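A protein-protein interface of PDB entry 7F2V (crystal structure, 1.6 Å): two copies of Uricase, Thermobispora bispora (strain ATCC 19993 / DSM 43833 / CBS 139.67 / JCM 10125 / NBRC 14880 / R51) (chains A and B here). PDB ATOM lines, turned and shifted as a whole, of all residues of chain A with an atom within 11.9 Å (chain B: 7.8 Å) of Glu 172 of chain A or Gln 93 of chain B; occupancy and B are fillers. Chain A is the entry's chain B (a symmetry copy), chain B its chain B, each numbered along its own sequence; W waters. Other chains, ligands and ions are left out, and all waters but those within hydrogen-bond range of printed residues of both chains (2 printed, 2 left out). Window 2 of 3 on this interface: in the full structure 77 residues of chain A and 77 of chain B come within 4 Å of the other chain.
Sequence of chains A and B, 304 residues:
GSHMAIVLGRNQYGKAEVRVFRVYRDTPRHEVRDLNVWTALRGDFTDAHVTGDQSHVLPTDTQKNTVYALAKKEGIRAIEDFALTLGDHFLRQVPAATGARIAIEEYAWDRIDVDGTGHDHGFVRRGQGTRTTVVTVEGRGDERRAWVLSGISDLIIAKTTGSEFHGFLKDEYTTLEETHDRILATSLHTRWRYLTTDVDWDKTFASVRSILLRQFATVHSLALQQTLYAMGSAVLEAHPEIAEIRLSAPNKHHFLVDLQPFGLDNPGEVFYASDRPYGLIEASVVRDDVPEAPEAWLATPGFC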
ATOM      1  N   PHE A 168     -29.139  10.940   2.370  1.00  0.00           N
ATOM      2  CA  PHE A 168     -28.918   9.708   3.087  1.00  0.00           C
ATOM      3  C   PHE A 168     -27.510   9.174   2.815  1.00  0.00           C
ATOM      4  O   PHE A 168     -26.796   9.641   1.924  1.00  0.00           O
ATOM      5  CB  PHE A 168     -29.982   8.678   2.696  1.00  0.00           C
ATOM      6  CG  PHE A 168     -30.247   8.586   1.213  1.00  0.00           C
ATOM      7  CD1 PHE A 168     -29.327   7.995   0.357  1.00  0.00           C
ATOM      8  CD2 PHE A 168     -31.445   9.042   0.683  1.00  0.00           C
ATOM      9  CE1 PHE A 168     -29.585   7.877  -0.999  1.00  0.00           C
ATOM     10  CE2 PHE A 168     -31.710   8.929  -0.671  1.00  0.00           C
ATOM     11  CZ  PHE A 168     -30.771   8.351  -1.517  1.00  0.00           C
ATOM     12  N   LEU A 169     -27.114   8.183   3.615  1.00  0.00           N
ATOM     13  CA  LEU A 169     -25.826   7.530   3.434  1.00  0.00           C
ATOM     14  C   LEU A 169     -25.834   6.728   2.138  1.00  0.00           C
ATOM     15  O   LEU A 169     -26.755   5.947   1.887  1.00  0.00           O
ATOM     16  CB  LEU A 169     -25.539   6.610   4.619  1.00  0.00           C
ATOM     17  CG  LEU A 169     -24.230   5.811   4.626  1.00  0.00           C
ATOM     18  CD1 LEU A 169     -23.034   6.732   4.751  1.00  0.00           C
ATOM     19  CD2 LEU A 169     -24.231   4.780   5.751  1.00  0.00           C
ATOM     20  N   LYS A 170     -24.824   6.914   1.302  1.00  0.00           N
ATOM     21  CA  LYS A 170     -24.782   6.189   0.045  1.00  0.00           C
ATOM     22  C   LYS A 170     -23.678   5.145   0.089  1.00  0.00           C
ATOM     23  O   LYS A 170     -22.561   5.411   0.546  1.00  0.00           O
ATOM     24  CB  LYS A 170     -24.633   7.130  -1.150  1.00  0.00           C
ATOM     25  CG  LYS A 170     -25.911   7.935  -1.373  1.00  0.00           C
ATOM     26  CD  LYS A 170     -25.686   9.246  -2.101  1.00  0.00           C
ATOM     27  CE  LYS A 170     -26.964   9.687  -2.806  1.00  0.00           C
ATOM     28  NZ  LYS A 170     -26.709  10.757  -3.804  1.00  0.00           N
ATOM     29  N   ASP A 171     -24.030   3.959  -0.366  1.00  0.00           N
ATOM     30  CA  ASP A 171     -23.266   2.733  -0.335  1.00  0.00           C
ATOM     31  C   ASP A 171     -22.883   2.388  -1.758  1.00  0.00           C
ATOM     32  O   ASP A 171     -23.477   2.890  -2.714  1.00  0.00           O
ATOM     33  CB  ASP A 171     -24.127   1.604   0.249  1.00  0.00           C
ATOM     34  CG  ASP A 171     -23.333   0.621   1.030  1.00  0.00           C
ATOM     35  OD1 ASP A 171     -22.139   0.893   1.259  1.00  0.00           O
ATOM     36  OD2 ASP A 171     -23.894  -0.423   1.414  1.00  0.00           O
ATOM     37  N   GLU A 172     -21.933   1.463  -1.896  1.00  0.00           N
ATOM     38  CA  GLU A 172     -21.678   0.916  -3.221  1.00  0.00           C
ATOM     39  C   GLU A 172     -22.851   0.091  -3.739  1.00  0.00           C
ATOM     40  O   GLU A 172     -22.847  -0.297  -4.911  1.00  0.00           O
ATOM     41  CB  GLU A 172     -20.402   0.067  -3.203  1.00  0.00           C
ATOM     42  CG  GLU A 172     -20.361  -0.980  -2.096  1.00  0.00           C
ATOM     43  CD  GLU A 172     -19.524  -0.544  -0.895  1.00  0.00           C
ATOM     44  OE1 GLU A 172     -19.812   0.526  -0.312  1.00  0.00           O
ATOM     45  OE2 GLU A 172     -18.577  -1.280  -0.533  1.00  0.00           O
ATOM     46  N   TYR A 173     -23.852  -0.177  -2.901  1.00  0.00           N
ATOM     47  CA  TYR A 173     -25.032  -0.922  -3.304  1.00  0.00           C
ATOM     48  C   TYR A 173     -26.265  -0.039  -3.406  1.00  0.00           C
ATOM     49  O   TYR A 173     -27.373  -0.561  -3.564  1.00  0.00           O
ATOM     50  CB  TYR A 173     -25.295  -2.064  -2.323  1.00  0.00           C
ATOM     51  CG  TYR A 173     -24.324  -3.218  -2.427  1.00  0.00           C
ATOM     52  CD1 TYR A 173     -23.397  -3.292  -3.459  1.00  0.00           C
ATOM     53  CD2 TYR A 173     -24.350  -4.245  -1.501  1.00  0.00           C
ATOM     54  CE1 TYR A 173     -22.514  -4.355  -3.547  1.00  0.00           C
ATOM     55  CE2 TYR A 173     -23.476  -5.304  -1.581  1.00  0.00           C
ATOM     56  CZ  TYR A 173     -22.563  -5.355  -2.602  1.00  0.00           C
ATOM     57  OH  TYR A 173     -21.700  -6.419  -2.664  1.00  0.00           O
ATOM     58  N   THR A 174     -26.104   1.278  -3.331  1.00  0.00           N
ATOM     59  CA  THR A 174     -27.236   2.195  -3.364  1.00  0.00           C
ATOM     60  C   THR A 174     -27.520   2.603  -4.807  1.00  0.00           C
ATOM     61  O   THR A 174     -26.635   3.130  -5.493  1.00  0.00           O
ATOM     62  CB  THR A 174     -26.964   3.427  -2.502  1.00  0.00           C
ATOM     63  OG1 THR A 174     -26.767   3.027  -1.144  1.00  0.00           O
ATOM     64  CG2 THR A 174     -28.144   4.395  -2.560  1.00  0.00           C
ATOM     65  N   THR A 175     -28.744   2.337  -5.261  1.00  0.00           N
ATOM     66  CA  THR A 175     -29.250   2.795  -6.550  1.00  0.00           C
ATOM     67  C   THR A 175     -30.330   3.858  -6.403  1.00  0.00           C
ATOM     68  O   THR A 175     -30.658   4.536  -7.387  1.00  0.00           O
ATOM     69  CB  THR A 175     -29.824   1.617  -7.355  1.00  0.00           C
ATOM     70  OG1 THR A 175     -30.819   0.958  -6.567  1.00  0.00           O
ATOM     71  CG2 THR A 175     -28.738   0.606  -7.731  1.00  0.00           C
ATOM     72  N   LEU A 176     -30.888   4.018  -5.208  1.00  0.00           N
ATOM     73  CA  LEU A 176     -32.012   4.921  -5.009  1.00  0.00           C
ATOM     74  C   LEU A 176     -31.579   6.361  -5.228  1.00  0.00           C
ATOM     75  O   LEU A 176     -30.558   6.805  -4.691  1.00  0.00           O
ATOM     76  CB  LEU A 176     -32.580   4.740  -3.597  1.00  0.00           C
ATOM     77  CG  LEU A 176     -33.720   5.652  -3.147  1.00  0.00           C
ATOM     78  CD1 LEU A 176     -35.013   5.246  -3.822  1.00  0.00           C
ATOM     79  CD2 LEU A 176     -33.862   5.630  -1.632  1.00  0.00           C
ATOM     80  N   LEU B  41     -32.024  -2.390  11.132  1.00  0.00           N
ATOM     81  CA  LEU B  41     -30.820  -1.852  11.754  1.00  0.00           C
ATOM     82  C   LEU B  41     -31.196  -1.079  13.005  1.00  0.00           C
ATOM     83  O   LEU B  41     -32.246  -0.428  13.051  1.00  0.00           O
ATOM     84  CB  LEU B  41     -30.063  -0.937  10.787  1.00  0.00           C
ATOM     85  CG  LEU B  41     -29.775  -1.542   9.408  1.00  0.00           C
ATOM     86  CD1 LEU B  41     -28.877  -0.609   8.592  1.00  0.00           C
ATOM     87  CD2 LEU B  41     -29.132  -2.924   9.548  1.00  0.00           C
ATOM     88  N   HIS B  56     -27.032   9.523   8.530  1.00  0.00           N
ATOM     89  CA  HIS B  56     -26.671   8.220   9.075  1.00  0.00           C
ATOM     90  C   HIS B  56     -27.415   7.065   8.419  1.00  0.00           C
ATOM     91  O   HIS B  56     -27.041   5.910   8.657  1.00  0.00           O
ATOM     92  CB  HIS B  56     -26.958   8.150  10.581  1.00  0.00           C
ATOM     93  CG  HIS B  56     -26.071   9.016  11.426  1.00  0.00           C
ATOM     94  ND1 HIS B  56     -26.112   8.989  12.803  1.00  0.00           N
ATOM     95  CD2 HIS B  56     -25.121   9.921  11.094  1.00  0.00           C
ATOM     96  CE1 HIS B  56     -25.231   9.849  13.285  1.00  0.00           C
ATOM     97  NE2 HIS B  56     -24.619  10.430  12.270  1.00  0.00           N
ATOM     98  N   LEU B  58     -28.763   4.399   5.899  1.00  0.00           N
ATOM     99  CA  LEU B  58     -28.672   3.650   4.650  1.00  0.00           C
ATOM    100  C   LEU B  58     -30.081   3.281   4.180  1.00  0.00           C
ATOM    101  O   LEU B  58     -30.833   2.660   4.943  1.00  0.00           O
ATOM    102  CB  LEU B  58     -27.819   2.398   4.845  1.00  0.00           C
ATOM    103  CG  LEU B  58     -27.532   1.575   3.587  1.00  0.00           C
ATOM    104  CD1 LEU B  58     -26.501   2.307   2.764  1.00  0.00           C
ATOM    105  CD2 LEU B  58     -27.075   0.138   3.923  1.00  0.00           C
ATOM    106  N   THR B  62     -31.517   0.141  -0.355  1.00  0.00           N
ATOM    107  CA  THR B  62     -30.165  -0.401  -0.456  1.00  0.00           C
ATOM    108  C   THR B  62     -30.061  -1.724   0.282  1.00  0.00           C
ATOM    109  O   THR B  62     -29.372  -2.648  -0.167  1.00  0.00           O
ATOM    110  CB  THR B  62     -29.154   0.599   0.101  1.00  0.00           C
ATOM    111  OG1 THR B  62     -29.221   1.808  -0.667  1.00  0.00           O
ATOM    112  CG2 THR B  62     -27.744   0.041   0.037  1.00  0.00           C
ATOM    113  N   ASN B  65     -31.334  -4.258  -2.071  1.00  0.00           N
ATOM    114  CA  ASN B  65     -30.283  -4.522  -3.063  1.00  0.00           C
ATOM    115  C   ASN B  65     -29.213  -5.442  -2.503  1.00  0.00           C
ATOM    116  O   ASN B  65     -28.690  -6.307  -3.214  1.00  0.00           O
ATOM    117  CB  ASN B  65     -29.618  -3.213  -3.516  1.00  0.00           C
ATOM    118  CG  ASN B  65     -30.499  -2.377  -4.425  1.00  0.00           C
ATOM    119  OD1 ASN B  65     -31.505  -2.848  -4.945  1.00  0.00           O
ATOM    120  ND2 ASN B  65     -30.099  -1.121  -4.646  1.00  0.00           N
ATOM    121  N   THR B  66     -28.838  -5.232  -1.241  1.00  0.00           N
ATOM    122  CA  THR B  66     -27.779  -6.025  -0.632  1.00  0.00           C
ATOM    123  C   THR B  66     -28.181  -7.489  -0.534  1.00  0.00           C
ATOM    124  O   THR B  66     -27.367  -8.385  -0.786  1.00  0.00           O
ATOM    125  CB  THR B  66     -27.455  -5.433   0.741  1.00  0.00           C
ATOM    126  OG1 THR B  66     -27.102  -4.047   0.569  1.00  0.00           O
ATOM    127  CG2 THR B  66     -26.315  -6.161   1.407  1.00  0.00           C
ATOM    128  N   LEU B  86     -25.344 -11.176   6.240  1.00  0.00           N
ATOM    129  CA  LEU B  86     -26.030  -9.910   6.026  1.00  0.00           C
ATOM    130  C   LEU B  86     -25.832  -8.969   7.207  1.00  0.00           C
ATOM    131  O   LEU B  86     -25.579  -7.772   7.019  1.00  0.00           O
ATOM    132  CB  LEU B  86     -27.518 -10.168   5.779  1.00  0.00           C
ATOM    133  CG  LEU B  86     -27.881 -10.652   4.367  1.00  0.00           C
ATOM    134  CD1 LEU B  86     -29.289 -11.210   4.325  1.00  0.00           C
ATOM    135  CD2 LEU B  86     -27.750  -9.496   3.365  1.00  0.00           C
ATOM    136  N   GLY B  87     -25.954  -9.489   8.431  1.00  0.00           N
ATOM    137  CA  GLY B  87     -25.775  -8.640   9.601  1.00  0.00           C
ATOM    138  C   GLY B  87     -24.391  -8.017   9.658  1.00  0.00           C
ATOM    139  O   GLY B  87     -24.245  -6.806   9.853  1.00  0.00           O
ATOM    140  N   ASP B  88     -23.348  -8.830   9.463  1.00  0.00           N
ATOM    141  CA  ASP B  88     -21.996  -8.275   9.476  1.00  0.00           C
ATOM    142  C   ASP B  88     -21.781  -7.303   8.323  1.00  0.00           C
ATOM    143  O   ASP B  88     -21.077  -6.299   8.473  1.00  0.00           O
ATOM    144  CB  ASP B  88     -20.960  -9.394   9.425  1.00  0.00           C
ATOM    145  CG  ASP B  88     -20.737 -10.047  10.779  1.00  0.00           C
ATOM    146  OD1 ASP B  88     -20.628  -9.320  11.802  1.00  0.00           O
ATOM    147  OD2 ASP B  88     -20.646 -11.295  10.809  1.00  0.00           O
ATOM    148  N   HIS B  89     -22.378  -7.574   7.163  1.00  0.00           N
ATOM    149  CA  HIS B  89     -22.230  -6.638   6.051  1.00  0.00           C
ATOM    150  C   HIS B  89     -22.797  -5.261   6.400  1.00  0.00           C
ATOM    151  O   HIS B  89     -22.157  -4.231   6.154  1.00  0.00           O
ATOM    152  CB  HIS B  89     -22.900  -7.188   4.792  1.00  0.00           C
ATOM    153  CG  HIS B  89     -22.858  -6.233   3.647  1.00  0.00           C
ATOM    154  ND1 HIS B  89     -21.855  -6.251   2.703  1.00  0.00           N
ATOM    155  CD2 HIS B  89     -23.673  -5.207   3.312  1.00  0.00           C
ATOM    156  CE1 HIS B  89     -22.068  -5.288   1.823  1.00  0.00           C
ATOM    157  NE2 HIS B  89     -23.165  -4.638   2.173  1.00  0.00           N
ATOM    158  N   PHE B  90     -24.005  -5.220   6.969  1.00  0.00           N
ATOM    159  CA  PHE B  90     -24.613  -3.927   7.274  1.00  0.00           C
ATOM    160  C   PHE B  90     -23.808  -3.173   8.323  1.00  0.00           C
ATOM    161  O   PHE B  90     -23.668  -1.946   8.247  1.00  0.00           O
ATOM    162  CB  PHE B  90     -26.062  -4.120   7.714  1.00  0.00           C
ATOM    163  CG  PHE B  90     -26.976  -4.519   6.584  1.00  0.00           C
ATOM    164  CD1 PHE B  90     -26.927  -3.837   5.377  1.00  0.00           C
ATOM    165  CD2 PHE B  90     -27.850  -5.591   6.708  1.00  0.00           C
ATOM    166  CE1 PHE B  90     -27.759  -4.191   4.308  1.00  0.00           C
ATOM    167  CE2 PHE B  90     -28.690  -5.952   5.645  1.00  0.00           C
ATOM    168  CZ  PHE B  90     -28.628  -5.254   4.442  1.00  0.00           C
ATOM    169  N   LEU B  91     -23.244  -3.887   9.297  1.00  0.00           N
ATOM    170  CA  LEU B  91     -22.423  -3.197  10.284  1.00  0.00           C
ATOM    171  C   LEU B  91     -21.171  -2.602   9.658  1.00  0.00           C
ATOM    172  O   LEU B  91     -20.725  -1.537  10.092  1.00  0.00           O
ATOM    173  CB  LEU B  91     -22.059  -4.137  11.429  1.00  0.00           C
ATOM    174  CG  LEU B  91     -23.267  -4.392  12.319  1.00  0.00           C
ATOM    175  CD1 LEU B  91     -22.989  -5.569  13.194  1.00  0.00           C
ATOM    176  CD2 LEU B  91     -23.576  -3.153  13.155  1.00  0.00           C
ATOM    177  N   ARG B  92     -20.603  -3.262   8.637  1.00  0.00           N
ATOM    178  CA  ARG B  92     -19.482  -2.679   7.903  1.00  0.00           C
ATOM    179  C   ARG B  92     -19.902  -1.434   7.135  1.00  0.00           C
ATOM    180  O   ARG B  92     -19.122  -0.484   7.010  1.00  0.00           O
ATOM    181  CB  ARG B  92     -18.885  -3.699   6.926  1.00  0.00           C
ATOM    182  CG  ARG B  92     -17.831  -4.613   7.497  1.00  0.00           C
ATOM    183  CD  ARG B  92     -17.009  -5.285   6.390  1.00  0.00           C
ATOM    184  NE  ARG B  92     -17.841  -6.091   5.484  1.00  0.00           N
ATOM    185  CZ  ARG B  92     -18.364  -7.279   5.784  1.00  0.00           C
ATOM    186  NH1 ARG B  92     -18.155  -7.824   6.975  1.00  0.00           N
ATOM    187  NH2 ARG B  92     -19.104  -7.922   4.890  1.00  0.00           N
ATOM    188  N   GLN B  93     -21.117  -1.431   6.583  1.00  0.00           N
ATOM    189  CA  GLN B  93     -21.526  -0.368   5.671  1.00  0.00           C
ATOM    190  C   GLN B  93     -22.147   0.831   6.370  1.00  0.00           C
ATOM    191  O   GLN B  93     -22.179   1.921   5.783  1.00  0.00           O
ATOM    192  CB  GLN B  93     -22.531  -0.903   4.644  1.00  0.00           C
ATOM    193  CG  GLN B  93     -21.988  -2.007   3.770  1.00  0.00           C
ATOM    194  CD  GLN B  93     -20.717  -1.600   3.064  1.00  0.00           C
ATOM    195  OE1 GLN B  93     -19.641  -2.115   3.351  1.00  0.00           O
ATOM    196  NE2 GLN B  93     -20.836  -0.675   2.127  1.00  0.00           N
ATOM    197  N   VAL B  94     -22.650   0.659   7.590  1.00  0.00           N
ATOM    198  CA  VAL B  94     -23.446   1.690   8.250  1.00  0.00           C
ATOM    199  C   VAL B  94     -22.787   2.016   9.583  1.00  0.00           C
ATOM    200  O   VAL B  94     -23.107   1.383  10.597  1.00  0.00           O
ATOM    201  CB  VAL B  94     -24.900   1.227   8.451  1.00  0.00           C
ATOM    202  CG1 VAL B  94     -25.773   2.356   8.991  1.00  0.00           C
ATOM    203  CG2 VAL B  94     -25.464   0.667   7.146  1.00  0.00           C
ATOM    204  N   PRO B  95     -21.870   2.985   9.630  1.00  0.00           N
ATOM    205  CA  PRO B  95     -21.126   3.225  10.879  1.00  0.00           C
ATOM    206  C   PRO B  95     -22.011   3.593  12.055  1.00  0.00           C
ATOM    207  O   PRO B  95     -21.662   3.289  13.201  1.00  0.00           O
ATOM    208  CB  PRO B  95     -20.180   4.374  10.509  1.00  0.00           C
ATOM    209  CG  PRO B  95     -20.098   4.348   9.009  1.00  0.00           C
ATOM    210  CD  PRO B  95     -21.407   3.833   8.516  1.00  0.00           C
ATOM    211  N   ALA B  96     -23.160   4.225  11.815  1.00  0.00           N
ATOM    212  CA  ALA B  96     -24.003   4.604  12.935  1.00  0.00           C
ATOM    213  C   ALA B  96     -24.753   3.416  13.526  1.00  0.00           C
ATOM    214  O   ALA B  96     -25.289   3.530  14.632  1.00  0.00           O
ATOM    215  CB  ALA B  96     -24.991   5.691  12.507  1.00  0.00           C
ATOM    216  N   ALA B  97     -24.803   2.287  12.823  1.00  0.00           N
ATOM    217  CA  ALA B  97     -25.496   1.118  13.341  1.00  0.00           C
ATOM    218  C   ALA B  97     -24.702   0.483  14.470  1.00  0.00           C
ATOM    219  O   ALA B  97     -23.482   0.319  14.376  1.00  0.00           O
ATOM    220  CB  ALA B  97     -25.717   0.088  12.230  1.00  0.00           C
ATOM    221  N   ARG B 140     -18.596  -4.771  16.587  1.00  0.00           N
ATOM    222  CA  ARG B 140     -17.569  -4.991  15.579  1.00  0.00           C
ATOM    223  C   ARG B 140     -16.278  -5.436  16.251  1.00  0.00           C
ATOM    224  O   ARG B 140     -16.047  -5.176  17.435  1.00  0.00           O
ATOM    225  CB  ARG B 140     -17.310  -3.716  14.754  1.00  0.00           C
ATOM    226  CG  ARG B 140     -18.555  -3.100  14.105  1.00  0.00           C
ATOM    227  CD  ARG B 140     -18.262  -1.704  13.553  1.00  0.00           C
ATOM    228  NE  ARG B 140     -19.361  -1.206  12.726  1.00  0.00           N
ATOM    229  CZ  ARG B 140     -20.438  -0.580  13.201  1.00  0.00           C
ATOM    230  NH1 ARG B 140     -20.568  -0.354  14.505  1.00  0.00           N
ATOM    231  NH2 ARG B 140     -21.392  -0.181  12.371  1.00  0.00           N
HETATM  232  O   HOH W   1     -33.497  -0.992  -6.009  1.00  0.00           O
HETATM  233  O   HOH W   2     -16.954  -0.983   1.953  1.00  0.00           O
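The backbone carbonyl oxygen (O) of Tyr 173 of chain A lies within hydrogen-bond range of the side-chain amide nitrogen (ND2) of Asn 65 of chain B (3.0 Å). The side-chain amide nitrogen (ND2) of Asn 65 of chain B is in hydrogen-bond range of the side-chain hydroxyl (OG1) of Thr 175 of chain A (2.9 Å). The side-chain amide nitrogen (NE2) of Gln 93 of chain B sits at hydrogen-bond distance from the side-chain carboxylate (OE1) of Glu 172 of chain A. The side-chain hydroxyl of Thr 62 of chain B lies within hydrogen-bond range of the side-chain hydroxyl of Thr 174 of chain A (2.8 Å). The side-chain amide nitrogen (NE2) of Gln 93 of chain B sits close to the side-chain carboxylate (OD2) of Asp 171 of chain A (3.2 Å).
The backbone carbonyl oxygen (O) of Thr 62 of chain B lies within hydrogen-bond range of the side-chain hydroxyl (OG1) of Thr 66 of chain B (2.8 Å). The side-chain hydroxyl of Thr 174 of chain A lies within hydrogen-bond range of the backbone NH of Asp 171 of chain A (3.0 Å).
CD1 of Leu 58 of chain B touches O of Leu 169 of chain A (3.8 Å). Gln 93 of chain B touches Leu 169 of chain A (O to CD2, 3.5 Å). Leu 58 of chain B touches Asp 171 of chain A. Asp 171 of chain A touches Thr 62 of chain B (CB to CG2, 3.9 Å). Tyr 173 of chain A touches Thr 62 of chain B. Tyr 173 of chain A touches Thr 66 of chain B (CD2 to OG1, 3.4 Å). CE2 of Tyr 173 of chain A touches CE1 of His 89 of chain B, 3.7 Å away. CD1 of Leu 58 of chain B touches OG1 of Thr 174 of chain A, at 3.98 Å.
Glu 172 of chain A touches just one residue of chain B: Gln 93 (2.9 Å). Of the printed residues of chain B, Thr 175 of chain A touches Asn 65. Of the printed residues of chain A, Leu 58 of chain B touches Leu 169 (3.8 Å), Asp 171 (3.5 Å) and Thr 174 (3.98 Å). His 89 of chain B touches just one residue of chain A: Tyr 173 (3.7 Å). Pro 95 of chain B touches none of the printed residues of chain A. Ala 96 of chain B touches none of the printed residues of chain A. The nearest residue of chain B that does not touch Glu 172 of chain A is His 89 of chain B (5.8 Å). The nearest printed residue of chain B that does not touch Thr 175 of chain A is Thr 62 of chain B (4.6 Å).
Of the 19 printed residues of chain B, 6 touch a printed residue of chain A. Hydrophobic or aromatic side chains of chain B within 4 Å of the printed part of chain A: Leu 58 and His 89. Along chain B the printed residues that touch a printed residue of chain A span positions 58 to 93. Printed residues of chain A that touch a printed residue of chain B: Leu 169, Asp 171, Glu 172, Tyr 173, Thr 174 and Thr 175. Among the printed residues, 13 pairs touch across the chains. Among the printed residues, no Asp or Glu carboxylate lies within 4 Å of a Lys or Arg side-chain nitrogen of the other chain.
No position is printed for both chains. Of the 13 pairs that touch across the chains among the printed residues, none has its exchanged pair printed and touching as well.
Water W1 lies within hydrogen-bond range of OD1 of Asn 65 of chain B (2.9 Å) and OG1 of Thr 175 of chain A (3.4 Å). Water W2 bridges OE2 of Glu 172 of chain A (3.0 Å) and OE1 of Gln 93 of chain B (3.2 Å).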
